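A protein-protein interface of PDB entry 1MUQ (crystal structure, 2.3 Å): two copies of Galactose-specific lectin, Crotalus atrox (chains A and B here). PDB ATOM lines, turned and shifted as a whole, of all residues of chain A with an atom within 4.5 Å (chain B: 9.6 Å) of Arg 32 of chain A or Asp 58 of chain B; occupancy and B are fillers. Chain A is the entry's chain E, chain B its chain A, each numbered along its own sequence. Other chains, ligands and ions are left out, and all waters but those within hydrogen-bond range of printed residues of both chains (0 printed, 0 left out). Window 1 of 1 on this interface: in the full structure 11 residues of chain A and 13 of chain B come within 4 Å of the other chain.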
ATOM      1  N   GLU A  28     -28.096 -10.588  13.472  1.00  0.00           N
ATOM      2  CA  GLU A  28     -27.237 -11.391  14.337  1.00  0.00           C
ATOM      3  C   GLU A  28     -26.035 -11.833  13.532  1.00  0.00           C
ATOM      4  O   GLU A  28     -24.896 -11.606  13.925  1.00  0.00           O
ATOM      5  CB  GLU A  28     -27.961 -12.663  14.816  1.00  0.00           C
ATOM      6  CG  GLU A  28     -28.014 -12.891  16.326  1.00  0.00           C
ATOM      7  CD  GLU A  28     -26.676 -12.741  17.050  1.00  0.00           C
ATOM      8  OE1 GLU A  28     -25.811 -13.634  16.960  1.00  0.00           O
ATOM      9  OE2 GLU A  28     -26.500 -11.713  17.729  1.00  0.00           O
ATOM     10  N   MET A  29     -26.314 -12.483  12.405  1.00  0.00           N
ATOM     11  CA  MET A  29     -25.272 -12.998  11.536  1.00  0.00           C
ATOM     12  C   MET A  29     -24.336 -11.918  11.052  1.00  0.00           C
ATOM     13  O   MET A  29     -23.126 -12.130  10.972  1.00  0.00           O
ATOM     14  CB  MET A  29     -25.892 -13.748  10.358  1.00  0.00           C
ATOM     15  CG  MET A  29     -26.503 -15.074  10.783  1.00  0.00           C
ATOM     16  SD  MET A  29     -25.440 -15.932  11.989  1.00  0.00           S
ATOM     17  CE  MET A  29     -23.960 -16.190  11.025  1.00  0.00           C
ATOM     18  N   PHE A  30     -24.883 -10.753  10.742  1.00  0.00           N
ATOM     19  CA  PHE A  30     -24.038  -9.666  10.300  1.00  0.00           C
ATOM     20  C   PHE A  30     -23.114  -9.261  11.457  1.00  0.00           C
ATOM     21  O   PHE A  30     -21.931  -8.989  11.246  1.00  0.00           O
ATOM     22  CB  PHE A  30     -24.885  -8.482   9.843  1.00  0.00           C
ATOM     23  CG  PHE A  30     -24.069  -7.292   9.424  1.00  0.00           C
ATOM     24  CD1 PHE A  30     -23.533  -6.429  10.374  1.00  0.00           C
ATOM     25  CD2 PHE A  30     -23.805  -7.056   8.084  1.00  0.00           C
ATOM     26  CE1 PHE A  30     -22.750  -5.347   9.995  1.00  0.00           C
ATOM     27  CE2 PHE A  30     -23.023  -5.977   7.698  1.00  0.00           C
ATOM     28  CZ  PHE A  30     -22.494  -5.122   8.658  1.00  0.00           C
ATOM     29  N   CYS A  31     -23.642  -9.218  12.679  1.00  0.00           N
ATOM     30  CA  CYS A  31     -22.801  -8.868  13.825  1.00  0.00           C
ATOM     31  C   CYS A  31     -21.738  -9.947  14.036  1.00  0.00           C
ATOM     32  O   CYS A  31     -20.562  -9.642  14.194  1.00  0.00           O
ATOM     33  CB  CYS A  31     -23.623  -8.733  15.110  1.00  0.00           C
ATOM     34  SG  CYS A  31     -24.783  -7.333  15.162  1.00  0.00           S
ATOM     35  N   ARG A  32     -22.167 -11.205  14.037  1.00  0.00           N
ATOM     36  CA  ARG A  32     -21.260 -12.327  14.224  1.00  0.00           C
ATOM     37  C   ARG A  32     -20.159 -12.338  13.169  1.00  0.00           C
ATOM     38  O   ARG A  32     -19.035 -12.728  13.446  1.00  0.00           O
ATOM     39  CB  ARG A  32     -22.028 -13.655  14.153  1.00  0.00           C
ATOM     40  CG  ARG A  32     -23.145 -13.799  15.171  1.00  0.00           C
ATOM     41  CD  ARG A  32     -22.909 -14.987  16.086  1.00  0.00           C
ATOM     42  NE  ARG A  32     -23.958 -16.000  15.991  1.00  0.00           N
ATOM     43  CZ  ARG A  32     -23.988 -16.962  15.078  1.00  0.00           C
ATOM     44  NH1 ARG A  32     -23.027 -17.048  14.177  1.00  0.00           N
ATOM     45  NH2 ARG A  32     -24.973 -17.849  15.070  1.00  0.00           N
ATOM     46  N   LYS A  33     -20.485 -11.907  11.956  1.00  0.00           N
ATOM     47  CA  LYS A  33     -19.506 -11.898  10.883  1.00  0.00           C
ATOM     48  C   LYS A  33     -18.770 -10.572  10.721  1.00  0.00           C
ATOM     49  O   LYS A  33     -17.901 -10.450   9.863  1.00  0.00           O
ATOM     50  CB  LYS A  33     -20.172 -12.293   9.562  1.00  0.00           C
ATOM     51  CG  LYS A  33     -20.920 -13.624   9.618  1.00  0.00           C
ATOM     52  CD  LYS A  33     -20.058 -14.728  10.195  1.00  0.00           C
ATOM     53  CE  LYS A  33     -18.863 -15.028   9.301  1.00  0.00           C
ATOM     54  NZ  LYS A  33     -19.298 -15.557   7.975  1.00  0.00           N
ATOM     55  N   TYR A  34     -19.112  -9.575  11.532  1.00  0.00           N
ATOM     56  CA  TYR A  34     -18.416  -8.301  11.437  1.00  0.00           C
ATOM     57  C   TYR A  34     -16.984  -8.521  11.932  1.00  0.00           C
ATOM     58  O   TYR A  34     -16.022  -8.010  11.364  1.00  0.00           O
ATOM     59  CB  TYR A  34     -19.121  -7.237  12.268  1.00  0.00           C
ATOM     60  CG  TYR A  34     -18.442  -5.894  12.207  1.00  0.00           C
ATOM     61  CD1 TYR A  34     -17.383  -5.587  13.058  1.00  0.00           C
ATOM     62  CD2 TYR A  34     -18.864  -4.921  11.299  1.00  0.00           C
ATOM     63  CE1 TYR A  34     -16.757  -4.335  13.012  1.00  0.00           C
ATOM     64  CE2 TYR A  34     -18.246  -3.669  11.243  1.00  0.00           C
ATOM     65  CZ  TYR A  34     -17.199  -3.381  12.100  1.00  0.00           C
ATOM     66  OH  TYR A  34     -16.603  -2.139  12.055  1.00  0.00           O
ATOM     67  N   LYS A  35     -16.858  -9.295  12.997  1.00  0.00           N
ATOM     68  CA  LYS A  35     -15.559  -9.649  13.542  1.00  0.00           C
ATOM     69  C   LYS A  35     -15.841 -10.706  14.597  1.00  0.00           C
ATOM     70  O   LYS A  35     -16.928 -10.738  15.173  1.00  0.00           O
ATOM     71  CB  LYS A  35     -14.853  -8.435  14.160  1.00  0.00           C
ATOM     72  CG  LYS A  35     -14.909  -8.406  15.659  1.00  0.00           C
ATOM     73  CD  LYS A  35     -13.906  -7.450  16.216  1.00  0.00           C
ATOM     74  CE  LYS A  35     -13.619  -7.799  17.652  1.00  0.00           C
ATOM     75  NZ  LYS A  35     -13.027  -9.159  17.745  1.00  0.00           N
ATOM     76  N   CYS A  38     -18.724 -10.824  18.150  1.00  0.00           N
ATOM     77  CA  CYS A  38     -19.835  -9.876  18.131  1.00  0.00           C
ATOM     78  C   CYS A  38     -21.197 -10.545  18.072  1.00  0.00           C
ATOM     79  O   CYS A  38     -21.351 -11.638  17.536  1.00  0.00           O
ATOM     80  CB  CYS A  38     -19.761  -8.964  16.914  1.00  0.00           C
ATOM     81  SG  CYS A  38     -18.193  -8.136  16.572  1.00  0.00           S
ATOM     82  N   HIS A  39     -22.190  -9.855  18.606  1.00  0.00           N
ATOM     83  CA  HIS A  39     -23.557 -10.354  18.583  1.00  0.00           C
ATOM     84  C   HIS A  39     -24.454  -9.149  18.627  1.00  0.00           C
ATOM     85  O   HIS A  39     -23.981  -8.024  18.740  1.00  0.00           O
ATOM     86  CB  HIS A  39     -23.867 -11.198  19.821  1.00  0.00           C
ATOM     87  CG  HIS A  39     -23.221 -12.541  19.819  1.00  0.00           C
ATOM     88  ND1 HIS A  39     -22.037 -12.800  20.473  1.00  0.00           N
ATOM     89  CD2 HIS A  39     -23.601 -13.709  19.249  1.00  0.00           C
ATOM     90  CE1 HIS A  39     -21.715 -14.068  20.308  1.00  0.00           C
ATOM     91  NE2 HIS A  39     -22.648 -14.641  19.569  1.00  0.00           N
ATOM     92  N   LEU B   5      -7.930  -7.865  15.281  1.00  0.00           N
ATOM     93  CA  LEU B   5      -9.307  -7.899  14.813  1.00  0.00           C
ATOM     94  C   LEU B   5      -9.840  -9.226  14.279  1.00  0.00           C
ATOM     95  O   LEU B   5     -11.043  -9.469  14.309  1.00  0.00           O
ATOM     96  CB  LEU B   5      -9.517  -6.787  13.787  1.00  0.00           C
ATOM     97  CG  LEU B   5      -9.935  -5.453  14.432  1.00  0.00           C
ATOM     98  CD1 LEU B   5      -9.037  -5.115  15.616  1.00  0.00           C
ATOM     99  CD2 LEU B   5      -9.884  -4.351  13.394  1.00  0.00           C
ATOM    100  N   TRP B   7      -9.217 -12.092  15.572  1.00  0.00           N
ATOM    101  CA  TRP B   7      -9.158 -13.049  16.663  1.00  0.00           C
ATOM    102  C   TRP B   7     -10.363 -12.874  17.566  1.00  0.00           C
ATOM    103  O   TRP B   7     -10.922 -11.782  17.657  1.00  0.00           O
ATOM    104  CB  TRP B   7      -7.888 -12.850  17.484  1.00  0.00           C
ATOM    105  CG  TRP B   7      -6.642 -13.330  16.801  1.00  0.00           C
ATOM    106  CD1 TRP B   7      -6.083 -12.834  15.654  1.00  0.00           C
ATOM    107  CD2 TRP B   7      -5.809 -14.415  17.218  1.00  0.00           C
ATOM    108  NE1 TRP B   7      -4.954 -13.548  15.329  1.00  0.00           N
ATOM    109  CE2 TRP B   7      -4.761 -14.525  16.271  1.00  0.00           C
ATOM    110  CE3 TRP B   7      -5.847 -15.308  18.294  1.00  0.00           C
ATOM    111  CZ2 TRP B   7      -3.763 -15.492  16.371  1.00  0.00           C
ATOM    112  CZ3 TRP B   7      -4.849 -16.275  18.393  1.00  0.00           C
ATOM    113  CH2 TRP B   7      -3.822 -16.357  17.434  1.00  0.00           C
ATOM    114  N   LEU B   8     -10.760 -13.957  18.231  1.00  0.00           N
ATOM    115  CA  LEU B   8     -11.893 -13.927  19.143  1.00  0.00           C
ATOM    116  C   LEU B   8     -11.435 -13.694  20.566  1.00  0.00           C
ATOM    117  O   LEU B   8     -10.717 -14.519  21.131  1.00  0.00           O
ATOM    118  CB  LEU B   8     -12.646 -15.247  19.092  1.00  0.00           C
ATOM    119  CG  LEU B   8     -13.596 -15.513  20.259  1.00  0.00           C
ATOM    120  CD1 LEU B   8     -14.843 -14.655  20.098  1.00  0.00           C
ATOM    121  CD2 LEU B   8     -13.978 -16.993  20.286  1.00  0.00           C
ATOM    122  N   ILE B  17      -9.235 -19.701  14.525  1.00  0.00           N
ATOM    123  CA  ILE B  17      -9.161 -20.965  13.809  1.00  0.00           C
ATOM    124  C   ILE B  17      -8.298 -20.763  12.594  1.00  0.00           C
ATOM    125  O   ILE B  17      -8.458 -19.791  11.862  1.00  0.00           O
ATOM    126  CB  ILE B  17     -10.524 -21.496  13.269  1.00  0.00           C
ATOM    127  CG1 ILE B  17     -11.607 -20.443  13.424  1.00  0.00           C
ATOM    128  CG2 ILE B  17     -10.851 -22.847  13.896  1.00  0.00           C
ATOM    129  CD1 ILE B  17     -11.505 -19.354  12.409  1.00  0.00           C
ATOM    130  N   ASN B  19      -7.406 -22.536   9.167  1.00  0.00           N
ATOM    131  CA  ASN B  19      -7.990 -23.556   8.309  1.00  0.00           C
ATOM    132  C   ASN B  19      -6.986 -24.553   7.755  1.00  0.00           C
ATOM    133  O   ASN B  19      -7.368 -25.603   7.241  1.00  0.00           O
ATOM    134  CB  ASN B  19      -8.763 -22.877   7.184  1.00  0.00           C
ATOM    135  CG  ASN B  19      -9.785 -21.873   7.713  1.00  0.00           C
ATOM    136  OD1 ASN B  19     -10.752 -22.244   8.382  1.00  0.00           O
ATOM    137  ND2 ASN B  19      -9.563 -20.592   7.425  1.00  0.00           N
ATOM    138  N   LEU B  50     -19.389 -23.086  23.835  1.00  0.00           N
ATOM    139  CA  LEU B  50     -20.430 -22.507  23.001  1.00  0.00           C
ATOM    140  C   LEU B  50     -19.942 -21.326  22.170  1.00  0.00           C
ATOM    141  O   LEU B  50     -20.253 -21.233  20.989  1.00  0.00           O
ATOM    142  CB  LEU B  50     -21.618 -22.091  23.874  1.00  0.00           C
ATOM    143  CG  LEU B  50     -22.254 -23.254  24.649  1.00  0.00           C
ATOM    144  CD1 LEU B  50     -23.424 -22.749  25.488  1.00  0.00           C
ATOM    145  CD2 LEU B  50     -22.721 -24.330  23.667  1.00  0.00           C
ATOM    146  N   GLU B  51     -19.169 -20.436  22.784  1.00  0.00           N
ATOM    147  CA  GLU B  51     -18.645 -19.265  22.090  1.00  0.00           C
ATOM    148  C   GLU B  51     -17.725 -19.738  20.965  1.00  0.00           C
ATOM    149  O   GLU B  51     -17.822 -19.292  19.816  1.00  0.00           O
ATOM    150  CB  GLU B  51     -17.872 -18.383  23.083  1.00  0.00           C
ATOM    151  CG  GLU B  51     -17.215 -17.131  22.498  1.00  0.00           C
ATOM    152  CD  GLU B  51     -18.162 -15.942  22.359  1.00  0.00           C
ATOM    153  OE1 GLU B  51     -19.021 -15.940  21.451  1.00  0.00           O
ATOM    154  OE2 GLU B  51     -18.043 -14.998  23.167  1.00  0.00           O
ATOM    155  N   ILE B  52     -16.836 -20.656  21.310  1.00  0.00           N
ATOM    156  CA  ILE B  52     -15.881 -21.209  20.353  1.00  0.00           C
ATOM    157  C   ILE B  52     -16.570 -21.992  19.246  1.00  0.00           C
ATOM    158  O   ILE B  52     -16.234 -21.846  18.074  1.00  0.00           O
ATOM    159  CB  ILE B  52     -14.888 -22.134  21.068  1.00  0.00           C
ATOM    160  CG1 ILE B  52     -13.920 -21.284  21.896  1.00  0.00           C
ATOM    161  CG2 ILE B  52     -14.192 -23.038  20.071  1.00  0.00           C
ATOM    162  CD1 ILE B  52     -13.166 -20.243  21.095  1.00  0.00           C
ATOM    163  N   ALA B  53     -17.526 -22.832  19.628  1.00  0.00           N
ATOM    164  CA  ALA B  53     -18.259 -23.638  18.662  1.00  0.00           C
ATOM    165  C   ALA B  53     -18.914 -22.722  17.635  1.00  0.00           C
ATOM    166  O   ALA B  53     -18.794 -22.942  16.430  1.00  0.00           O
ATOM    167  CB  ALA B  53     -19.311 -24.480  19.370  1.00  0.00           C
ATOM    168  N   GLU B  54     -19.582 -21.680  18.122  1.00  0.00           N
ATOM    169  CA  GLU B  54     -20.259 -20.721  17.254  1.00  0.00           C
ATOM    170  C   GLU B  54     -19.262 -19.944  16.392  1.00  0.00           C
ATOM    171  O   GLU B  54     -19.537 -19.646  15.228  1.00  0.00           O
ATOM    172  CB  GLU B  54     -21.074 -19.756  18.111  1.00  0.00           C
ATOM    173  CG  GLU B  54     -21.784 -18.670  17.352  1.00  0.00           C
ATOM    174  CD  GLU B  54     -22.568 -17.755  18.279  1.00  0.00           C
ATOM    175  OE1 GLU B  54     -21.940 -17.114  19.150  1.00  0.00           O
ATOM    176  OE2 GLU B  54     -23.809 -17.684  18.143  1.00  0.00           O
ATOM    177  N   TYR B  55     -18.103 -19.628  16.974  1.00  0.00           N
ATOM    178  CA  TYR B  55     -17.041 -18.893  16.286  1.00  0.00           C
ATOM    179  C   TYR B  55     -16.486 -19.687  15.106  1.00  0.00           C
ATOM    180  O   TYR B  55     -16.328 -19.171  13.992  1.00  0.00           O
ATOM    181  CB  TYR B  55     -15.905 -18.597  17.261  1.00  0.00           C
ATOM    182  CG  TYR B  55     -14.616 -18.204  16.588  1.00  0.00           C
ATOM    183  CD1 TYR B  55     -13.449 -18.957  16.772  1.00  0.00           C
ATOM    184  CD2 TYR B  55     -14.563 -17.098  15.739  1.00  0.00           C
ATOM    185  CE1 TYR B  55     -12.264 -18.615  16.123  1.00  0.00           C
ATOM    186  CE2 TYR B  55     -13.383 -16.748  15.080  1.00  0.00           C
ATOM    187  CZ  TYR B  55     -12.240 -17.511  15.276  1.00  0.00           C
ATOM    188  OH  TYR B  55     -11.078 -17.157  14.623  1.00  0.00           O
ATOM    189  N   ILE B  56     -16.167 -20.946  15.367  1.00  0.00           N
ATOM    190  CA  ILE B  56     -15.638 -21.815  14.330  1.00  0.00           C
ATOM    191  C   ILE B  56     -16.652 -22.026  13.201  1.00  0.00           C
ATOM    192  O   ILE B  56     -16.302 -21.963  12.026  1.00  0.00           O
ATOM    193  CB  ILE B  56     -15.231 -23.165  14.931  1.00  0.00           C
ATOM    194  CG1 ILE B  56     -14.063 -22.946  15.894  1.00  0.00           C
ATOM    195  CG2 ILE B  56     -14.855 -24.140  13.829  1.00  0.00           C
ATOM    196  CD1 ILE B  56     -13.704 -24.154  16.710  1.00  0.00           C
ATOM    197  N   SER B  57     -17.907 -22.273  13.556  1.00  0.00           N
ATOM    198  CA  SER B  57     -18.943 -22.484  12.553  1.00  0.00           C
ATOM    199  C   SER B  57     -19.079 -21.280  11.632  1.00  0.00           C
ATOM    200  O   SER B  57     -19.383 -21.433  10.450  1.00  0.00           O
ATOM    201  CB  SER B  57     -20.292 -22.737  13.223  1.00  0.00           C
ATOM    202  OG  SER B  57     -20.155 -23.673  14.274  1.00  0.00           O
ATOM    203  N   ASP B  58     -18.853 -20.081  12.166  1.00  0.00           N
ATOM    204  CA  ASP B  58     -18.991 -18.871  11.359  1.00  0.00           C
ATOM    205  C   ASP B  58     -17.753 -18.517  10.570  1.00  0.00           C
ATOM    206  O   ASP B  58     -17.850 -17.991   9.465  1.00  0.00           O
ATOM    207  CB  ASP B  58     -19.332 -17.651  12.224  1.00  0.00           C
ATOM    208  CG  ASP B  58     -20.576 -17.842  13.060  1.00  0.00           C
ATOM    209  OD1 ASP B  58     -21.513 -18.538  12.614  1.00  0.00           O
ATOM    210  OD2 ASP B  58     -20.616 -17.271  14.170  1.00  0.00           O
ATOM    211  N   TYR B  59     -16.589 -18.796  11.139  1.00  0.00           N
ATOM    212  CA  TYR B  59     -15.342 -18.426  10.494  1.00  0.00           C
ATOM    213  C   TYR B  59     -14.492 -19.517   9.876  1.00  0.00           C
ATOM    214  O   TYR B  59     -13.641 -19.235   9.039  1.00  0.00           O
ATOM    215  CB  TYR B  59     -14.497 -17.622  11.479  1.00  0.00           C
ATOM    216  CG  TYR B  59     -15.077 -16.260  11.768  1.00  0.00           C
ATOM    217  CD1 TYR B  59     -16.099 -16.090  12.710  1.00  0.00           C
ATOM    218  CD2 TYR B  59     -14.631 -15.142  11.066  1.00  0.00           C
ATOM    219  CE1 TYR B  59     -16.661 -14.827  12.942  1.00  0.00           C
ATOM    220  CE2 TYR B  59     -15.178 -13.888  11.288  1.00  0.00           C
ATOM    221  CZ  TYR B  59     -16.191 -13.728  12.219  1.00  0.00           C
ATOM    222  OH  TYR B  59     -16.721 -12.469  12.409  1.00  0.00           O
ATOM    223  N   HIS B  60     -14.702 -20.759  10.288  1.00  0.00           N
ATOM    224  CA  HIS B  60     -13.923 -21.850   9.732  1.00  0.00           C
ATOM    225  C   HIS B  60     -14.283 -22.041   8.268  1.00  0.00           C
ATOM    226  O   HIS B  60     -15.445 -22.240   7.919  1.00  0.00           O
ATOM    227  CB  HIS B  60     -14.177 -23.146  10.509  1.00  0.00           C
ATOM    228  CG  HIS B  60     -13.508 -24.349   9.918  1.00  0.00           C
ATOM    229  ND1 HIS B  60     -12.238 -24.310   9.381  1.00  0.00           N
ATOM    230  CD2 HIS B  60     -13.916 -25.636   9.816  1.00  0.00           C
ATOM    231  CE1 HIS B  60     -11.892 -25.519   8.977  1.00  0.00           C
ATOM    232  NE2 HIS B  60     -12.893 -26.342   9.231  1.00  0.00           N
ATOM    233  N   LYS B  61     -13.273 -21.955   7.414  1.00  0.00           N
ATOM    234  CA  LYS B  61     -13.465 -22.148   5.990  1.00  0.00           C
ATOM    235  C   LYS B  61     -13.115 -23.605   5.727  1.00  0.00           C
ATOM    236  O   LYS B  61     -11.976 -23.943   5.398  1.00  0.00           O
ATOM    237  CB  LYS B  61     -12.553 -21.201   5.207  1.00  0.00           C
ATOM    238  CG  LYS B  61     -12.882 -19.732   5.459  1.00  0.00           C
ATOM    239  CD  LYS B  61     -11.886 -18.782   4.814  1.00  0.00           C
ATOM    240  CE  LYS B  61     -12.249 -17.338   5.124  1.00  0.00           C
ATOM    241  NZ  LYS B  61     -11.271 -16.372   4.555  1.00  0.00           N
ATOM    242  N   GLY B  62     -14.112 -24.465   5.908  1.00  0.00           N
ATOM    243  CA  GLY B  62     -13.926 -25.888   5.712  1.00  0.00           C
ATOM    244  C   GLY B  62     -14.973 -26.656   6.492  1.00  0.00           C
ATOM    245  O   GLY B  62     -15.939 -26.069   6.974  1.00  0.00           O
ATOM    246  N   GLY B 114     -21.223 -29.478  15.644  1.00  0.00           N
ATOM    247  CA  GLY B 114     -21.197 -28.028  15.585  1.00  0.00           C
ATOM    248  C   GLY B 114     -19.976 -27.509  16.318  1.00  0.00           C
ATOM    249  O   GLY B 114     -19.962 -26.370  16.791  1.00  0.00           O
ATOM    250  N   TYR B 115     -18.954 -28.357  16.421  1.00  0.00           N
ATOM    251  CA  TYR B 115     -17.700 -28.008  17.087  1.00  0.00           C
ATOM    252  C   TYR B 115     -17.856 -27.789  18.577  1.00  0.00           C
ATOM    253  O   TYR B 115     -17.034 -27.123  19.208  1.00  0.00           O
ATOM    254  CB  TYR B 115     -17.096 -26.758  16.458  1.00  0.00           C
ATOM    255  CG  TYR B 115     -16.794 -26.937  14.997  1.00  0.00           C
ATOM    256  CD1 TYR B 115     -17.506 -26.236  14.019  1.00  0.00           C
ATOM    257  CD2 TYR B 115     -15.798 -27.820  14.587  1.00  0.00           C
ATOM    258  CE1 TYR B 115     -17.224 -26.417  12.665  1.00  0.00           C
ATOM    259  CE2 TYR B 115     -15.511 -28.005  13.251  1.00  0.00           C
ATOM    260  CZ  TYR B 115     -16.219 -27.304  12.293  1.00  0.00           C
ATOM    261  OH  TYR B 115     -15.890 -27.488  10.968  1.00  0.00           O
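O of Trp 7 of chain B sits at hydrogen-bond distance from NZ of Lys 35 of chain A (3.4 Å).
OE2 of Glu 54 of chain B is in salt-bridge range of NE of Arg 32 of chain A (2.7 Å).
NE2 of His 39 of chain A sits at hydrogen-bond distance from OE1 of Glu 54 of chain B, at 2.6 Å.
The guanidinium group (NH1) of Arg 32 of chain A is in salt-bridge range of the side-chain carboxylate (OD2) of Asp 58 of chain B (2.4 Å).
O of Asp 58 of chain B lies close to NZ of Lys 33 of chain A.
The side-chain hydroxyl (OH) of Tyr 59 of chain B sits at hydrogen-bond distance from the backbone carbonyl oxygen (O) of Arg 32 of chain A, 2.5 Å away.
OH of Tyr 59 of chain B sits close to O of Lys 33 of chain A (3.5 Å).
N of Lys 35 of chain A lies close to OH of Tyr 59 of chain B.
The side-chain carboxylate of Glu 28 of chain A is in salt-bridge range of the guanidinium group of Arg 32 of chain A.
The side-chain sulfur of Met 29 of chain A lies close to the guanidinium group of Arg 32 of chain A, 3.4 Å away.
CE of Met 29 of chain A touches OD1 of Asp 58 of chain B (3.7 Å).
Tyr 59 of chain B touches Tyr 34 of chain A (OH to N, 3.9 Å).
Lys 35 of chain A touches Leu 5 of chain B.
His 39 of chain A touches Glu 51 of chain B (CE1 to OE1, 3.5 Å).
Met 29 of chain A touches just one residue of chain B: Asp 58 (3.7 Å).
Cys 31 of chain A touches none of the printed residues of chain B.
Arg 32 of chain A touches three residues of chain B.
Of chain B, only Asp 58 and Tyr 59 come within 4 Å of Lys 33 of chain A.
Printed residues of chain A within 4 Å of Leu 5 of chain B: Lys 35.
Printed residues of chain A within 4 Å of Trp 7 of chain B: Lys 35.
Ile 52 of chain B touches none of the printed residues of chain A.
Printed residues of chain A within 4 Å of Glu 54 of chain B: Arg 32 (2.7 Å) and His 39 (2.6 Å).
Printed residues of chain A within 4 Å of Asp 58 of chain B: Met 29 (3.7 Å), Arg 32 (2.4 Å) and Lys 33 (3.1 Å).
The nearest residue of chain B that does not touch Arg 32 of chain A is Tyr 55 of chain B (6.2 Å).
Hydrophobic or aromatic side chains of chain B within 4 Å of the printed part of chain A: Tyr 59.
Hydrophobic or aromatic side chains of chain A within 4 Å of the printed part of chain B: Met 29 and His 39.
Among the printed residues, 12 pairs touch across the chains.
Among the printed residues, Asp or Glu carboxylates within 4 Å of a Lys or Arg side-chain nitrogen of the other chain: Arg 32 of chain A with Glu 54 of chain B (2.7 Å) and Arg 32 of chain A with Asp 58 of chain B (2.4 Å).
No position is printed for both chains.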
